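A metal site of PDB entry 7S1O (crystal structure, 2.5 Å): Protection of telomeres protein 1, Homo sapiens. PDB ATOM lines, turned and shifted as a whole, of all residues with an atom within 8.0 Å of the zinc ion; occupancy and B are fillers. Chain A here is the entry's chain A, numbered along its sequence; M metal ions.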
ATOM      1  N   HIS A  60      -4.278 -27.177 -28.201  1.00  0.00           N
ATOM      2  CA  HIS A  60      -4.069 -25.839 -28.755  1.00  0.00           C
ATOM      3  C   HIS A  60      -4.984 -24.842 -28.050  1.00  0.00           C
ATOM      4  O   HIS A  60      -6.185 -25.114 -27.887  1.00  0.00           O
ATOM      5  CB  HIS A  60      -4.331 -25.834 -30.262  1.00  0.00           C
ATOM      6  CG  HIS A  60      -4.316 -24.471 -30.870  1.00  0.00           C
ATOM      7  ND1 HIS A  60      -3.161 -23.717 -30.992  1.00  0.00           N
ATOM      8  CD2 HIS A  60      -5.302 -23.718 -31.420  1.00  0.00           C
ATOM      9  CE1 HIS A  60      -3.453 -22.569 -31.570  1.00  0.00           C
ATOM     10  NE2 HIS A  60      -4.737 -22.544 -31.842  1.00  0.00           N
ATOM     11  N   CYS A  61      -4.422 -23.705 -27.634  1.00  0.00           N
ATOM     12  CA  CYS A  61      -5.263 -22.644 -27.101  1.00  0.00           C
ATOM     13  C   CYS A  61      -5.601 -21.644 -28.197  1.00  0.00           C
ATOM     14  O   CYS A  61      -4.682 -21.133 -28.856  1.00  0.00           O
ATOM     15  CB  CYS A  61      -4.580 -21.914 -25.953  1.00  0.00           C
ATOM     16  SG  CYS A  61      -5.551 -20.543 -25.280  1.00  0.00           S
ATOM     17  N   PRO A  62      -6.877 -21.329 -28.400  1.00  0.00           N
ATOM     18  CA  PRO A  62      -7.238 -20.340 -29.434  1.00  0.00           C
ATOM     19  C   PRO A  62      -6.764 -18.929 -29.130  1.00  0.00           C
ATOM     20  O   PRO A  62      -6.875 -18.060 -30.005  1.00  0.00           O
ATOM     21  CB  PRO A  62      -8.767 -20.415 -29.467  1.00  0.00           C
ATOM     22  CG  PRO A  62      -9.169 -21.004 -28.154  1.00  0.00           C
ATOM     23  CD  PRO A  62      -8.058 -21.928 -27.764  1.00  0.00           C
ATOM     24  N   LYS A  63      -6.263 -18.655 -27.924  1.00  0.00           N
ATOM     25  CA  LYS A  63      -5.807 -17.307 -27.594  1.00  0.00           C
ATOM     26  C   LYS A  63      -4.288 -17.222 -27.551  1.00  0.00           C
ATOM     27  O   LYS A  63      -3.676 -16.688 -28.486  1.00  0.00           O
ATOM     28  CB  LYS A  63      -6.382 -16.857 -26.247  1.00  0.00           C
ATOM     29  CG  LYS A  63      -7.544 -15.907 -26.373  1.00  0.00           C
ATOM     30  CD  LYS A  63      -8.159 -15.587 -25.034  1.00  0.00           C
ATOM     31  CE  LYS A  63      -9.487 -16.307 -24.859  1.00  0.00           C
ATOM     32  NZ  LYS A  63     -10.246 -15.827 -23.669  1.00  0.00           N
ATOM     33  N   CYS A  64      -3.680 -17.729 -26.482  1.00  0.00           N
ATOM     34  CA  CYS A  64      -2.234 -17.643 -26.351  1.00  0.00           C
ATOM     35  C   CYS A  64      -1.520 -18.411 -27.457  1.00  0.00           C
ATOM     36  O   CYS A  64      -0.317 -18.221 -27.635  1.00  0.00           O
ATOM     37  CB  CYS A  64      -1.776 -18.181 -25.006  1.00  0.00           C
ATOM     38  SG  CYS A  64      -1.999 -19.959 -24.833  1.00  0.00           S
ATOM     39  N   HIS A  65      -2.241 -19.268 -28.180  1.00  0.00           N
ATOM     40  CA  HIS A  65      -1.735 -20.072 -29.285  1.00  0.00           C
ATOM     41  C   HIS A  65      -0.668 -21.062 -28.847  1.00  0.00           C
ATOM     42  O   HIS A  65       0.090 -21.574 -29.682  1.00  0.00           O
ATOM     43  CB  HIS A  65      -1.202 -19.187 -30.419  1.00  0.00           C
ATOM     44  CG  HIS A  65      -2.267 -18.659 -31.329  1.00  0.00           C
ATOM     45  ND1 HIS A  65      -2.838 -17.418 -31.164  1.00  0.00           N
ATOM     46  CD2 HIS A  65      -2.869 -19.219 -32.405  1.00  0.00           C
ATOM     47  CE1 HIS A  65      -3.747 -17.231 -32.104  1.00  0.00           C
ATOM     48  NE2 HIS A  65      -3.783 -18.306 -32.872  1.00  0.00           N
ATOM     49  N   LEU A  66      -0.604 -21.346 -27.545  1.00  0.00           N
ATOM     50  CA  LEU A  66       0.310 -22.359 -27.041  1.00  0.00           C
ATOM     51  C   LEU A  66      -0.053 -23.733 -27.599  1.00  0.00           C
ATOM     52  O   LEU A  66      -1.190 -23.995 -28.005  1.00  0.00           O
ATOM     53  CB  LEU A  66       0.256 -22.418 -25.513  1.00  0.00           C
ATOM     54  CG  LEU A  66       1.414 -21.856 -24.686  1.00  0.00           C
ATOM     55  CD1 LEU A  66       1.684 -20.405 -25.041  1.00  0.00           C
ATOM     56  CD2 LEU A  66       1.118 -22.011 -23.201  1.00  0.00           C
ATOM     57  N   LEU A  67       0.942 -24.617 -27.604  1.00  0.00           N
ATOM     58  CA  LEU A  67       0.751 -26.020 -27.923  1.00  0.00           C
ATOM     59  C   LEU A  67       1.376 -26.836 -26.804  1.00  0.00           C
ATOM     60  O   LEU A  67       2.545 -26.624 -26.467  1.00  0.00           O
ATOM     61  CB  LEU A  67       1.372 -26.381 -29.270  1.00  0.00           C
ATOM     62  CG  LEU A  67       0.644 -25.874 -30.519  1.00  0.00           C
ATOM     63  CD1 LEU A  67       1.398 -26.247 -31.776  1.00  0.00           C
ATOM     64  CD2 LEU A  67      -0.778 -26.409 -30.560  1.00  0.00           C
ATOM     65  N   GLN A  68       0.609 -27.753 -26.231  1.00  0.00           N
ATOM     66  CA  GLN A  68       1.116 -28.646 -25.207  1.00  0.00           C
ATOM     67  C   GLN A  68       0.696 -30.078 -25.524  1.00  0.00           C
ATOM     68  O   GLN A  68      -0.217 -30.321 -26.314  1.00  0.00           O
ATOM     69  CB  GLN A  68       0.637 -28.246 -23.795  1.00  0.00           C
ATOM     70  CG  GLN A  68      -0.801 -28.642 -23.461  1.00  0.00           C
ATOM     71  CD  GLN A  68      -1.255 -28.031 -22.156  1.00  0.00           C
ATOM     72  OE1 GLN A  68      -1.209 -26.813 -21.973  1.00  0.00           O
ATOM     73  NE2 GLN A  68      -1.703 -28.883 -21.234  1.00  0.00           N
ATOM     74  N   GLY A 181      -8.138 -27.115 -20.214  1.00  0.00           N
ATOM     75  CA  GLY A 181      -8.142 -25.675 -20.263  1.00  0.00           C
ATOM     76  C   GLY A 181      -6.737 -25.097 -20.314  1.00  0.00           C
ATOM     77  O   GLY A 181      -5.763 -25.783 -19.989  1.00  0.00           O
ATOM     78  N   CYS A 182      -6.623 -23.838 -20.723  1.00  0.00           N
ATOM     79  CA  CYS A 182      -5.326 -23.190 -20.820  1.00  0.00           C
ATOM     80  C   CYS A 182      -4.864 -22.721 -19.454  1.00  0.00           C
ATOM     81  O   CYS A 182      -5.588 -22.006 -18.756  1.00  0.00           O
ATOM     82  CB  CYS A 182      -5.376 -22.011 -21.783  1.00  0.00           C
ATOM     83  SG  CYS A 182      -3.801 -21.175 -21.947  1.00  0.00           S
ATOM     84  N   LYS A 183      -3.640 -23.106 -19.070  1.00  0.00           N
ATOM     85  CA  LYS A 183      -3.118 -22.771 -17.750  1.00  0.00           C
ATOM     86  C   LYS A 183      -2.659 -21.323 -17.639  1.00  0.00           C
ATOM     87  O   LYS A 183      -2.278 -20.892 -16.545  1.00  0.00           O
ATOM     88  CB  LYS A 183      -1.948 -23.696 -17.395  1.00  0.00           C
ATOM     89  CG  LYS A 183      -2.378 -24.997 -16.755  1.00  0.00           C
ATOM     90  CD  LYS A 183      -1.197 -25.724 -16.143  1.00  0.00           C
ATOM     91  CE  LYS A 183      -1.192 -25.590 -14.624  1.00  0.00           C
ATOM     92  NZ  LYS A 183      -0.511 -24.349 -14.165  1.00  0.00           N
ATOM     93  N   GLN A 184      -2.671 -20.560 -18.727  1.00  0.00           N
ATOM     94  CA  GLN A 184      -2.190 -19.185 -18.723  1.00  0.00           C
ATOM     95  C   GLN A 184      -3.248 -18.161 -19.114  1.00  0.00           C
ATOM     96  O   GLN A 184      -3.183 -17.017 -18.656  1.00  0.00           O
ATOM     97  CB  GLN A 184      -0.983 -19.035 -19.653  1.00  0.00           C
ATOM     98  CG  GLN A 184      -0.076 -20.261 -19.687  1.00  0.00           C
ATOM     99  CD  GLN A 184       1.116 -20.134 -18.753  1.00  0.00           C
ATOM    100  OE1 GLN A 184       1.820 -19.128 -18.773  1.00  0.00           O
ATOM    101  NE2 GLN A 184       1.339 -21.159 -17.937  1.00  0.00           N
ATOM    102  N   CYS A 185      -4.224 -18.539 -19.949  1.00  0.00           N
ATOM    103  CA  CYS A 185      -5.300 -17.639 -20.321  1.00  0.00           C
ATOM    104  C   CYS A 185      -6.523 -17.773 -19.420  1.00  0.00           C
ATOM    105  O   CYS A 185      -7.408 -16.915 -19.484  1.00  0.00           O
ATOM    106  CB  CYS A 185      -5.719 -17.872 -21.777  1.00  0.00           C
ATOM    107  SG  CYS A 185      -4.428 -17.550 -23.008  1.00  0.00           S
ATOM    108  N   SER A 186      -6.583 -18.795 -18.580  1.00  0.00           N
ATOM    109  CA  SER A 186      -7.733 -19.032 -17.729  1.00  0.00           C
ATOM    110  C   SER A 186      -7.615 -18.249 -16.425  1.00  0.00           C
ATOM    111  O   SER A 186      -6.511 -18.028 -15.903  1.00  0.00           O
ATOM    112  CB  SER A 186      -7.899 -20.517 -17.411  1.00  0.00           C
ATOM    113  OG  SER A 186      -7.907 -21.285 -18.605  1.00  0.00           O
ATOM    114  N   VAL A 215     -10.526 -21.044 -20.366  1.00  0.00           N
ATOM    115  CA  VAL A 215     -10.366 -20.962 -21.815  1.00  0.00           C
ATOM    116  C   VAL A 215     -10.086 -22.374 -22.325  1.00  0.00           C
ATOM    117  O   VAL A 215      -8.983 -22.899 -22.062  1.00  0.00           O
ATOM    118  CB  VAL A 215      -9.256 -19.987 -22.210  1.00  0.00           C
ATOM    119  CG1 VAL A 215      -9.009 -20.035 -23.717  1.00  0.00           C
ATOM    120  CG2 VAL A 215      -9.615 -18.572 -21.773  1.00  0.00           C
ATOM    121  N   PRO A 216     -11.022 -23.022 -23.014  1.00  0.00           N
ATOM    122  CA  PRO A 216     -10.862 -24.455 -23.331  1.00  0.00           C
ATOM    123  C   PRO A 216      -9.842 -24.682 -24.440  1.00  0.00           C
ATOM    124  O   PRO A 216      -9.853 -24.008 -25.462  1.00  0.00           O
ATOM    125  CB  PRO A 216     -12.270 -24.876 -23.763  1.00  0.00           C
ATOM    126  CG  PRO A 216     -12.873 -23.619 -24.311  1.00  0.00           C
ATOM    127  CD  PRO A 216     -12.304 -22.479 -23.504  1.00  0.00           C
ATOM    128  N   LEU A 217      -8.963 -25.655 -24.218  1.00  0.00           N
ATOM    129  CA  LEU A 217      -8.025 -26.076 -25.246  1.00  0.00           C
ATOM    130  C   LEU A 217      -8.746 -26.890 -26.314  1.00  0.00           C
ATOM    131  O   LEU A 217      -9.849 -27.416 -26.102  1.00  0.00           O
ATOM    132  CB  LEU A 217      -6.890 -26.892 -24.644  1.00  0.00           C
ATOM    133  CG  LEU A 217      -6.034 -26.168 -23.601  1.00  0.00           C
ATOM    134  CD1 LEU A 217      -4.956 -27.088 -23.037  1.00  0.00           C
ATOM    135  CD2 LEU A 217      -5.407 -24.922 -24.205  1.00  0.00           C
HETATM  136 ZN    ZN M   1      -4.020 -19.724 -23.739  1.00  0.00          ZN
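The side-chain sulfur of Cys 64 sits close to the backbone NH of Leu 66 (3.4 Å). N of Gln 184 sits close to SG of Cys 182 (3.5 Å). N of Cys 182 is in hydrogen-bond range of O of Val 215 (2.9 Å). The backbone carbonyl oxygen (O) of Cys 182 lies within hydrogen-bond range of the side-chain hydroxyl (OG) of Ser 186 (2.4 Å). N of Lys 63 sits close to SG of Cys 61, at 3.3 Å. N of Cys 61 sits at hydrogen-bond distance from O of Leu 66 (3.3 Å).
Within 4 Å of the zinc ion: Cys 61, Cys 64, Cys 182 and Cys 185. Along chain A the residues within 4 Å of the zinc ion span positions 61 to 185.
The side-chain sulfur (SG) of Cys 64 binds the zinc ion (2.3 Å). SG of Cys 182 binds the zinc ion (2.3 Å). The zinc ion is bound by SG of Cys 61. The side-chain sulfur (SG) of Cys 185 is bound to the zinc ion. The zinc ion has four donor atoms within binding distance.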
